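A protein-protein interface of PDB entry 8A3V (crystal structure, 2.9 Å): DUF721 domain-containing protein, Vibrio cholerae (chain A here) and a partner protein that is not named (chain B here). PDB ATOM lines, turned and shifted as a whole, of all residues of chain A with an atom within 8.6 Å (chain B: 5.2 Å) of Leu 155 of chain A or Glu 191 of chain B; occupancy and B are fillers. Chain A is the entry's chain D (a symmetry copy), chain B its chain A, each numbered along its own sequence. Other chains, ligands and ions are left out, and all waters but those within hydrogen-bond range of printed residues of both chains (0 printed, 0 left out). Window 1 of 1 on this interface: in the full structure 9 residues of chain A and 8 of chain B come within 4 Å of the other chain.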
ATOM      1  N   PRO A 124       3.788  20.747 -34.283  1.00  0.00           N
ATOM      2  CA  PRO A 124       5.041  20.271 -33.689  1.00  0.00           C
ATOM      3  C   PRO A 124       5.008  19.532 -32.341  1.00  0.00           C
ATOM      4  O   PRO A 124       6.102  19.474 -31.772  1.00  0.00           O
ATOM      5  CB  PRO A 124       5.854  21.562 -33.544  1.00  0.00           C
ATOM      6  CG  PRO A 124       4.810  22.663 -33.383  1.00  0.00           C
ATOM      7  CD  PRO A 124       3.468  22.118 -33.837  1.00  0.00           C
ATOM      8  N   PRO A 125       3.908  18.952 -31.782  1.00  0.00           N
ATOM      9  CA  PRO A 125       4.053  18.266 -30.481  1.00  0.00           C
ATOM     10  C   PRO A 125       4.935  17.033 -30.604  1.00  0.00           C
ATOM     11  O   PRO A 125       4.724  16.235 -31.516  1.00  0.00           O
ATOM     12  CB  PRO A 125       2.619  17.889 -30.102  1.00  0.00           C
ATOM     13  CG  PRO A 125       1.735  18.710 -30.996  1.00  0.00           C
ATOM     14  CD  PRO A 125       2.513  18.884 -32.261  1.00  0.00           C
ATOM     15  N   LEU A 126       5.947  16.898 -29.736  1.00  0.00           N
ATOM     16  CA  LEU A 126       6.829  15.738 -29.803  1.00  0.00           C
ATOM     17  C   LEU A 126       6.182  14.528 -29.167  1.00  0.00           C
ATOM     18  O   LEU A 126       5.444  14.661 -28.194  1.00  0.00           O
ATOM     19  CB  LEU A 126       8.223  16.021 -29.209  1.00  0.00           C
ATOM     20  CG  LEU A 126       9.402  15.218 -29.791  1.00  0.00           C
ATOM     21  CD1 LEU A 126       9.375  15.183 -31.290  1.00  0.00           C
ATOM     22  CD2 LEU A 126      10.713  15.807 -29.359  1.00  0.00           C
ATOM     23  N   SER A 127       6.419  13.348 -29.740  1.00  0.00           N
ATOM     24  CA  SER A 127       5.821  12.117 -29.244  1.00  0.00           C
ATOM     25  C   SER A 127       6.713  11.386 -28.258  1.00  0.00           C
ATOM     26  O   SER A 127       7.937  11.496 -28.316  1.00  0.00           O
ATOM     27  CB  SER A 127       5.486  11.189 -30.409  1.00  0.00           C
ATOM     28  OG  SER A 127       4.982   9.939 -29.960  1.00  0.00           O
ATOM     29  N   ALA A 131      10.978  10.349 -28.063  1.00  0.00           N
ATOM     30  CA  ALA A 131      11.813  10.384 -26.866  1.00  0.00           C
ATOM     31  C   ALA A 131      12.462   9.021 -26.637  1.00  0.00           C
ATOM     32  O   ALA A 131      13.641   8.959 -26.302  1.00  0.00           O
ATOM     33  CB  ALA A 131      10.979  10.775 -25.653  1.00  0.00           C
ATOM     34  N   LEU A 134      15.199   8.545 -29.221  1.00  0.00           N
ATOM     35  CA  LEU A 134      16.313   9.427 -28.871  1.00  0.00           C
ATOM     36  C   LEU A 134      17.163   8.807 -27.757  1.00  0.00           C
ATOM     37  O   LEU A 134      18.390   8.864 -27.817  1.00  0.00           O
ATOM     38  CB  LEU A 134      15.800  10.812 -28.446  1.00  0.00           C
ATOM     39  CG  LEU A 134      15.290  11.693 -29.576  1.00  0.00           C
ATOM     40  CD1 LEU A 134      14.513  12.866 -29.037  1.00  0.00           C
ATOM     41  CD2 LEU A 134      16.416  12.160 -30.457  1.00  0.00           C
ATOM     42  N   LYS A 144      29.253  13.208 -25.221  1.00  0.00           N
ATOM     43  CA  LYS A 144      28.825  14.541 -25.630  1.00  0.00           C
ATOM     44  C   LYS A 144      27.487  14.493 -26.368  1.00  0.00           C
ATOM     45  O   LYS A 144      26.608  15.311 -26.108  1.00  0.00           O
ATOM     46  CB  LYS A 144      29.895  15.201 -26.515  1.00  0.00           C
ATOM     47  CG  LYS A 144      31.181  15.557 -25.781  1.00  0.00           C
ATOM     48  CD  LYS A 144      32.162  16.273 -26.707  1.00  0.00           C
ATOM     49  CE  LYS A 144      33.444  16.643 -26.004  1.00  0.00           C
ATOM     50  NZ  LYS A 144      34.418  17.283 -26.928  1.00  0.00           N
ATOM     51  N   VAL A 145      27.330  13.531 -27.275  1.00  0.00           N
ATOM     52  CA  VAL A 145      26.105  13.356 -28.052  1.00  0.00           C
ATOM     53  C   VAL A 145      24.982  12.759 -27.196  1.00  0.00           C
ATOM     54  O   VAL A 145      23.818  13.127 -27.349  1.00  0.00           O
ATOM     55  CB  VAL A 145      26.388  12.503 -29.300  1.00  0.00           C
ATOM     56  CG1 VAL A 145      25.128  12.310 -30.130  1.00  0.00           C
ATOM     57  CG2 VAL A 145      27.492  13.123 -30.137  1.00  0.00           C
ATOM     58  N   LYS A 147      24.414  13.268 -23.976  1.00  0.00           N
ATOM     59  CA  LYS A 147      23.816  14.344 -23.179  1.00  0.00           C
ATOM     60  C   LYS A 147      22.813  15.175 -23.992  1.00  0.00           C
ATOM     61  O   LYS A 147      21.761  15.538 -23.472  1.00  0.00           O
ATOM     62  CB  LYS A 147      24.901  15.261 -22.591  1.00  0.00           C
ATOM     63  CG  LYS A 147      25.702  14.641 -21.455  1.00  0.00           C
ATOM     64  CD  LYS A 147      26.754  15.614 -20.947  1.00  0.00           C
ATOM     65  CE  LYS A 147      27.602  15.030 -19.843  1.00  0.00           C
ATOM     66  NZ  LYS A 147      28.588  16.023 -19.334  1.00  0.00           N
ATOM     67  N   ARG A 148      23.127  15.465 -25.263  1.00  0.00           N
ATOM     68  CA  ARG A 148      22.239  16.237 -26.133  1.00  0.00           C
ATOM     69  C   ARG A 148      20.993  15.438 -26.516  1.00  0.00           C
ATOM     70  O   ARG A 148      19.898  15.997 -26.581  1.00  0.00           O
ATOM     71  CB  ARG A 148      22.987  16.723 -27.383  1.00  0.00           C
ATOM     72  CG  ARG A 148      24.039  17.803 -27.100  1.00  0.00           C
ATOM     73  CD  ARG A 148      23.413  19.126 -26.693  1.00  0.00           C
ATOM     74  NE  ARG A 148      24.403  20.099 -26.217  1.00  0.00           N
ATOM     75  CZ  ARG A 148      24.102  21.233 -25.589  1.00  0.00           C
ATOM     76  NH1 ARG A 148      22.835  21.556 -25.352  1.00  0.00           N
ATOM     77  NH2 ARG A 148      25.065  22.057 -25.194  1.00  0.00           N
ATOM     78  N   LEU A 149      21.151  14.124 -26.728  1.00  0.00           N
ATOM     79  CA  LEU A 149      20.036  13.242 -27.075  1.00  0.00           C
ATOM     80  C   LEU A 149      19.106  13.055 -25.884  1.00  0.00           C
ATOM     81  O   LEU A 149      17.890  13.057 -26.053  1.00  0.00           O
ATOM     82  CB  LEU A 149      20.553  11.890 -27.576  1.00  0.00           C
ATOM     83  CG  LEU A 149      21.149  11.919 -28.972  1.00  0.00           C
ATOM     84  CD1 LEU A 149      21.894  10.662 -29.273  1.00  0.00           C
ATOM     85  CD2 LEU A 149      20.079  12.153 -30.011  1.00  0.00           C
ATOM     86  N   GLN A 150      19.676  12.925 -24.672  1.00  0.00           N
ATOM     87  CA  GLN A 150      18.892  12.810 -23.441  1.00  0.00           C
ATOM     88  C   GLN A 150      18.163  14.126 -23.161  1.00  0.00           C
ATOM     89  O   GLN A 150      17.023  14.102 -22.707  1.00  0.00           O
ATOM     90  CB  GLN A 150      19.787  12.445 -22.248  1.00  0.00           C
ATOM     91  CG  GLN A 150      20.304  11.015 -22.283  1.00  0.00           C
ATOM     92  CD  GLN A 150      21.165  10.681 -21.090  1.00  0.00           C
ATOM     93  OE1 GLN A 150      21.785  11.542 -20.461  1.00  0.00           O
ATOM     94  NE2 GLN A 150      21.231   9.409 -20.757  1.00  0.00           N
ATOM     95  N   SER A 151      18.815  15.268 -23.453  1.00  0.00           N
ATOM     96  CA  SER A 151      18.223  16.591 -23.289  1.00  0.00           C
ATOM     97  C   SER A 151      17.034  16.746 -24.237  1.00  0.00           C
ATOM     98  O   SER A 151      15.981  17.225 -23.823  1.00  0.00           O
ATOM     99  CB  SER A 151      19.259  17.676 -23.556  1.00  0.00           C
ATOM    100  OG  SER A 151      20.271  17.679 -22.560  1.00  0.00           O
ATOM    101  N   LEU A 152      17.181  16.296 -25.487  1.00  0.00           N
ATOM    102  CA  LEU A 152      16.110  16.361 -26.475  1.00  0.00           C
ATOM    103  C   LEU A 152      14.953  15.428 -26.105  1.00  0.00           C
ATOM    104  O   LEU A 152      13.791  15.792 -26.280  1.00  0.00           O
ATOM    105  CB  LEU A 152      16.657  15.994 -27.851  1.00  0.00           C
ATOM    106  CG  LEU A 152      15.802  16.408 -29.015  1.00  0.00           C
ATOM    107  CD1 LEU A 152      15.583  17.919 -29.073  1.00  0.00           C
ATOM    108  CD2 LEU A 152      16.433  15.976 -30.290  1.00  0.00           C
ATOM    109  N   ALA A 153      15.271  14.237 -25.569  1.00  0.00           N
ATOM    110  CA  ALA A 153      14.263  13.271 -25.131  1.00  0.00           C
ATOM    111  C   ALA A 153      13.499  13.800 -23.911  1.00  0.00           C
ATOM    112  O   ALA A 153      12.299  13.561 -23.788  1.00  0.00           O
ATOM    113  CB  ALA A 153      14.922  11.943 -24.804  1.00  0.00           C
ATOM    114  N   ARG A 154      14.187  14.545 -23.031  1.00  0.00           N
ATOM    115  CA  ARG A 154      13.585  15.182 -21.859  1.00  0.00           C
ATOM    116  C   ARG A 154      12.596  16.263 -22.313  1.00  0.00           C
ATOM    117  O   ARG A 154      11.531  16.420 -21.718  1.00  0.00           O
ATOM    118  CB  ARG A 154      14.670  15.806 -20.965  1.00  0.00           C
ATOM    119  CG  ARG A 154      15.335  14.832 -19.987  1.00  0.00           C
ATOM    120  CD  ARG A 154      16.248  15.538 -19.012  1.00  0.00           C
ATOM    121  NE  ARG A 154      17.572  15.766 -19.588  1.00  0.00           N
ATOM    122  CZ  ARG A 154      18.612  16.245 -18.914  1.00  0.00           C
ATOM    123  NH1 ARG A 154      18.497  16.550 -17.628  1.00  0.00           N
ATOM    124  NH2 ARG A 154      19.778  16.419 -19.520  1.00  0.00           N
ATOM    125  N   LEU A 155      12.947  16.998 -23.375  1.00  0.00           N
ATOM    126  CA  LEU A 155      12.087  18.026 -23.946  1.00  0.00           C
ATOM    127  C   LEU A 155      10.832  17.436 -24.602  1.00  0.00           C
ATOM    128  O   LEU A 155       9.843  18.144 -24.745  1.00  0.00           O
ATOM    129  CB  LEU A 155      12.859  18.857 -24.973  1.00  0.00           C
ATOM    130  CG  LEU A 155      13.963  19.748 -24.420  1.00  0.00           C
ATOM    131  CD1 LEU A 155      14.733  20.411 -25.537  1.00  0.00           C
ATOM    132  CD2 LEU A 155      13.410  20.785 -23.472  1.00  0.00           C
ATOM    133  N   ALA A 156      10.873  16.154 -25.008  1.00  0.00           N
ATOM    134  CA  ALA A 156       9.740  15.480 -25.636  1.00  0.00           C
ATOM    135  C   ALA A 156       8.610  15.207 -24.647  1.00  0.00           C
ATOM    136  O   ALA A 156       8.748  14.354 -23.781  1.00  0.00           O
ATOM    137  CB  ALA A 156      10.190  14.181 -26.274  1.00  0.00           C
ATOM    138  N   LYS A 157       7.489  15.917 -24.801  1.00  0.00           N
ATOM    139  CA  LYS A 157       6.287  15.820 -23.961  1.00  0.00           C
ATOM    140  C   LYS A 157       5.226  14.885 -24.560  1.00  0.00           C
ATOM    141  O   LYS A 157       4.997  14.920 -25.765  1.00  0.00           O
ATOM    142  CB  LYS A 157       5.679  17.216 -23.694  1.00  0.00           C
ATOM    143  CG  LYS A 157       5.688  18.164 -24.891  1.00  0.00           C
ATOM    144  CD  LYS A 157       5.114  19.536 -24.573  1.00  0.00           C
ATOM    145  CE  LYS A 157       5.139  20.379 -25.814  1.00  0.00           C
ATOM    146  NZ  LYS A 157       4.457  21.683 -25.616  1.00  0.00           N
ATOM    147  N   ALA A 158       4.519  14.124 -23.714  1.00  0.00           N
ATOM    148  CA  ALA A 158       3.482  13.195 -24.159  1.00  0.00           C
ATOM    149  C   ALA A 158       2.144  13.823 -24.526  1.00  0.00           C
ATOM    150  O   ALA A 158       1.200  13.834 -23.726  1.00  0.00           O
ATOM    151  CB  ALA A 158       3.259  12.117 -23.138  1.00  0.00           C
ATOM    152  N   THR B 186      24.635  19.878 -33.922  1.00  0.00           N
ATOM    153  CA  THR B 186      23.333  19.880 -34.577  1.00  0.00           C
ATOM    154  C   THR B 186      22.225  19.801 -33.527  1.00  0.00           C
ATOM    155  O   THR B 186      21.277  20.583 -33.574  1.00  0.00           O
ATOM    156  CB  THR B 186      23.237  18.709 -35.562  1.00  0.00           C
ATOM    157  OG1 THR B 186      24.313  18.783 -36.499  1.00  0.00           O
ATOM    158  CG2 THR B 186      21.895  18.660 -36.271  1.00  0.00           C
ATOM    159  N   LEU B 187      22.367  18.884 -32.557  1.00  0.00           N
ATOM    160  CA  LEU B 187      21.380  18.700 -31.498  1.00  0.00           C
ATOM    161  C   LEU B 187      21.321  19.907 -30.577  1.00  0.00           C
ATOM    162  O   LEU B 187      20.236  20.280 -30.151  1.00  0.00           O
ATOM    163  CB  LEU B 187      21.670  17.435 -30.694  1.00  0.00           C
ATOM    164  CG  LEU B 187      21.567  16.127 -31.458  1.00  0.00           C
ATOM    165  CD1 LEU B 187      22.124  14.994 -30.648  1.00  0.00           C
ATOM    166  CD2 LEU B 187      20.146  15.847 -31.881  1.00  0.00           C
ATOM    167  N   GLU B 188      22.474  20.524 -30.288  1.00  0.00           N
ATOM    168  CA  GLU B 188      22.554  21.725 -29.454  1.00  0.00           C
ATOM    169  C   GLU B 188      21.790  22.867 -30.128  1.00  0.00           C
ATOM    170  O   GLU B 188      21.050  23.585 -29.461  1.00  0.00           O
ATOM    171  CB  GLU B 188      24.026  22.115 -29.228  1.00  0.00           C
ATOM    172  CG  GLU B 188      24.250  23.399 -28.447  1.00  0.00           C
ATOM    173  CD  GLU B 188      25.691  23.881 -28.402  1.00  0.00           C
ATOM    174  OE1 GLU B 188      25.918  25.029 -27.955  1.00  0.00           O
ATOM    175  OE2 GLU B 188      26.593  23.119 -28.819  1.00  0.00           O
ATOM    176  N   ARG B 189      21.939  22.998 -31.456  1.00  0.00           N
ATOM    177  CA  ARG B 189      21.266  24.022 -32.248  1.00  0.00           C
ATOM    178  C   ARG B 189      19.757  23.806 -32.236  1.00  0.00           C
ATOM    179  O   ARG B 189      19.008  24.755 -32.015  1.00  0.00           O
ATOM    180  CB  ARG B 189      21.808  24.020 -33.687  1.00  0.00           C
ATOM    181  CG  ARG B 189      21.503  25.292 -34.459  1.00  0.00           C
ATOM    182  CD  ARG B 189      22.224  26.505 -33.889  1.00  0.00           C
ATOM    183  NE  ARG B 189      23.686  26.380 -33.926  1.00  0.00           N
ATOM    184  CZ  ARG B 189      24.460  26.319 -32.845  1.00  0.00           C
ATOM    185  NH1 ARG B 189      25.778  26.220 -32.968  1.00  0.00           N
ATOM    186  NH2 ARG B 189      23.924  26.363 -31.634  1.00  0.00           N
ATOM    187  N   ILE B 190      19.313  22.555 -32.435  1.00  0.00           N
ATOM    188  CA  ILE B 190      17.891  22.210 -32.413  1.00  0.00           C
ATOM    189  C   ILE B 190      17.303  22.503 -31.034  1.00  0.00           C
ATOM    190  O   ILE B 190      16.229  23.092 -30.930  1.00  0.00           O
ATOM    191  CB  ILE B 190      17.685  20.734 -32.826  1.00  0.00           C
ATOM    192  CG1 ILE B 190      18.079  20.515 -34.300  1.00  0.00           C
ATOM    193  CG2 ILE B 190      16.249  20.284 -32.571  1.00  0.00           C
ATOM    194  CD1 ILE B 190      18.149  19.074 -34.721  1.00  0.00           C
ATOM    195  N   GLU B 191      18.036  22.140 -29.980  1.00  0.00           N
ATOM    196  CA  GLU B 191      17.631  22.377 -28.598  1.00  0.00           C
ATOM    197  C   GLU B 191      17.436  23.867 -28.334  1.00  0.00           C
ATOM    198  O   GLU B 191      16.438  24.251 -27.729  1.00  0.00           O
ATOM    199  CB  GLU B 191      18.671  21.789 -27.633  1.00  0.00           C
ATOM    200  CG  GLU B 191      18.352  21.995 -26.164  1.00  0.00           C
ATOM    201  CD  GLU B 191      19.255  21.248 -25.202  1.00  0.00           C
ATOM    202  OE1 GLU B 191      19.125  21.472 -23.978  1.00  0.00           O
ATOM    203  OE2 GLU B 191      20.091  20.438 -25.666  1.00  0.00           O
ATOM    204  N   LEU B 192      18.358  24.706 -28.821  1.00  0.00           N
ATOM    205  CA  LEU B 192      18.259  26.153 -28.649  1.00  0.00           C
ATOM    206  C   LEU B 192      17.042  26.725 -29.366  1.00  0.00           C
ATOM    207  O   LEU B 192      16.370  27.595 -28.819  1.00  0.00           O
ATOM    208  CB  LEU B 192      19.539  26.850 -29.126  1.00  0.00           C
ATOM    209  CG  LEU B 192      20.768  26.643 -28.252  1.00  0.00           C
ATOM    210  CD1 LEU B 192      21.982  27.282 -28.874  1.00  0.00           C
ATOM    211  CD2 LEU B 192      20.554  27.198 -26.856  1.00  0.00           C
ATOM    212  N   LEU B 193      16.745  26.228 -30.574  1.00  0.00           N
ATOM    213  CA  LEU B 193      15.586  26.685 -31.341  1.00  0.00           C
ATOM    214  C   LEU B 193      14.285  26.304 -30.641  1.00  0.00           C
ATOM    215  O   LEU B 193      13.349  27.100 -30.597  1.00  0.00           O
ATOM    216  CB  LEU B 193      15.614  26.092 -32.756  1.00  0.00           C
ATOM    217  CG  LEU B 193      16.757  26.566 -33.643  1.00  0.00           C
ATOM    218  CD1 LEU B 193      16.799  25.784 -34.941  1.00  0.00           C
ATOM    219  CD2 LEU B 193      16.654  28.061 -33.910  1.00  0.00           C
ATOM    220  N   TYR B 194      14.239  25.097 -30.072  1.00  0.00           N
ATOM    221  CA  TYR B 194      13.055  24.615 -29.370  1.00  0.00           C
ATOM    222  C   TYR B 194      12.792  25.352 -28.052  1.00  0.00           C
ATOM    223  O   TYR B 194      11.638  25.483 -27.649  1.00  0.00           O
ATOM    224  CB  TYR B 194      13.122  23.092 -29.169  1.00  0.00           C
ATOM    225  CG  TYR B 194      12.431  22.319 -30.271  1.00  0.00           C
ATOM    226  CD1 TYR B 194      11.078  22.023 -30.196  1.00  0.00           C
ATOM    227  CD2 TYR B 194      13.125  21.904 -31.399  1.00  0.00           C
ATOM    228  CE1 TYR B 194      10.434  21.327 -31.212  1.00  0.00           C
ATOM    229  CE2 TYR B 194      12.492  21.209 -32.421  1.00  0.00           C
ATOM    230  CZ  TYR B 194      11.147  20.922 -32.323  1.00  0.00           C
ATOM    231  OH  TYR B 194      10.521  20.226 -33.329  1.00  0.00           O
ATOM    232  N   LYS B 195      13.846  25.853 -27.395  1.00  0.00           N
ATOM    233  CA  LYS B 195      13.697  26.599 -26.144  1.00  0.00           C
ATOM    234  C   LYS B 195      13.149  28.013 -26.384  1.00  0.00           C
ATOM    235  O   LYS B 195      12.446  28.551 -25.532  1.00  0.00           O
ATOM    236  CB  LYS B 195      15.035  26.681 -25.394  1.00  0.00           C
ATOM    237  CG  LYS B 195      15.440  25.399 -24.683  1.00  0.00           C
ATOM    238  CD  LYS B 195      16.772  25.573 -23.963  1.00  0.00           C
ATOM    239  CE  LYS B 195      17.216  24.324 -23.247  1.00  0.00           C
ATOM    240  NZ  LYS B 195      18.565  24.490 -22.641  1.00  0.00           N
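NH1 of Arg 148 of chain A lies within salt-bridge range of OE2 of Glu 191 of chain B (3.0 Å).
The side-chain carboxylate (OE1) of Glu 191 of chain B lies within salt-bridge range of the side-chain amino group (NZ) of Lys 195 of chain B. The side-chain hydroxyl of Ser 151 of chain A is in hydrogen-bond range of the guanidinium group of Arg 154 of chain A (3.3 Å). The backbone carbonyl oxygen (O) of Lys 147 of chain A lies within hydrogen-bond range of the side-chain hydroxyl (OG) of Ser 151 of chain A (2.8 Å).
Leu 187 of chain B touches Arg 148 of chain A. Arg 148 of chain A touches Glu 188 of chain B (CZ to CG, 3.6 Å). Leu 149 of chain A touches Leu 187 of chain B. CB of Ser 151 of chain A touches OE2 of Glu 191 of chain B (3.6 Å). Glu 191 of chain B touches Leu 155 of chain A (CG to CD1, 3.9999 Å).
Printed residues of chain B within 4 Å of Arg 148 of chain A: Leu 187, Glu 188 and Glu 191. Of the printed residues of chain B, Leu 149 of chain A touches Leu 187. Of the printed residues of chain B, Ser 151 of chain A touches Glu 191. Printed residues of chain B within 4 Å of Leu 155 of chain A: Glu 191 (3.9999 Å). Ala 156 of chain A touches none of the printed residues of chain B. Printed residues of chain A within 4 Å of Leu 187 of chain B: Arg 148 (3.6 Å) and Leu 149 (3.6 Å). Printed residues of chain A within 4 Å of Glu 188 of chain B: Arg 148. Arg 189 of chain B touches none of the printed residues of chain A. Printed residues of chain A within 4 Å of Glu 191 of chain B: Arg 148, Ser 151 and Leu 155.
Of the 10 printed residues of chain B, 3 touch a printed residue of chain A. Printed residues of chain B that touch a printed residue of chain A: Leu 187, Glu 188 and Glu 191. Hydrophobic or aromatic side chains of chain B that line the printed part of chain A: Leu 187. Of the 20 printed residues of chain A, 4 touch a printed residue of chain B. Printed residues of chain A that touch a printed residue of chain B: Arg 148, Leu 149, Ser 151 and Leu 155. Hydrophobic or aromatic side chains of chain A within 4 Å of the printed part of chain B: Leu 149 and Leu 155. Among the printed residues, 6 pairs touch across the chains. Among the printed residues, Asp or Glu carboxylates within 4 Å of a Lys or Arg side-chain nitrogen of the other chain: Arg 148 of chain A with Glu 191 of chain B (3.0 Å).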
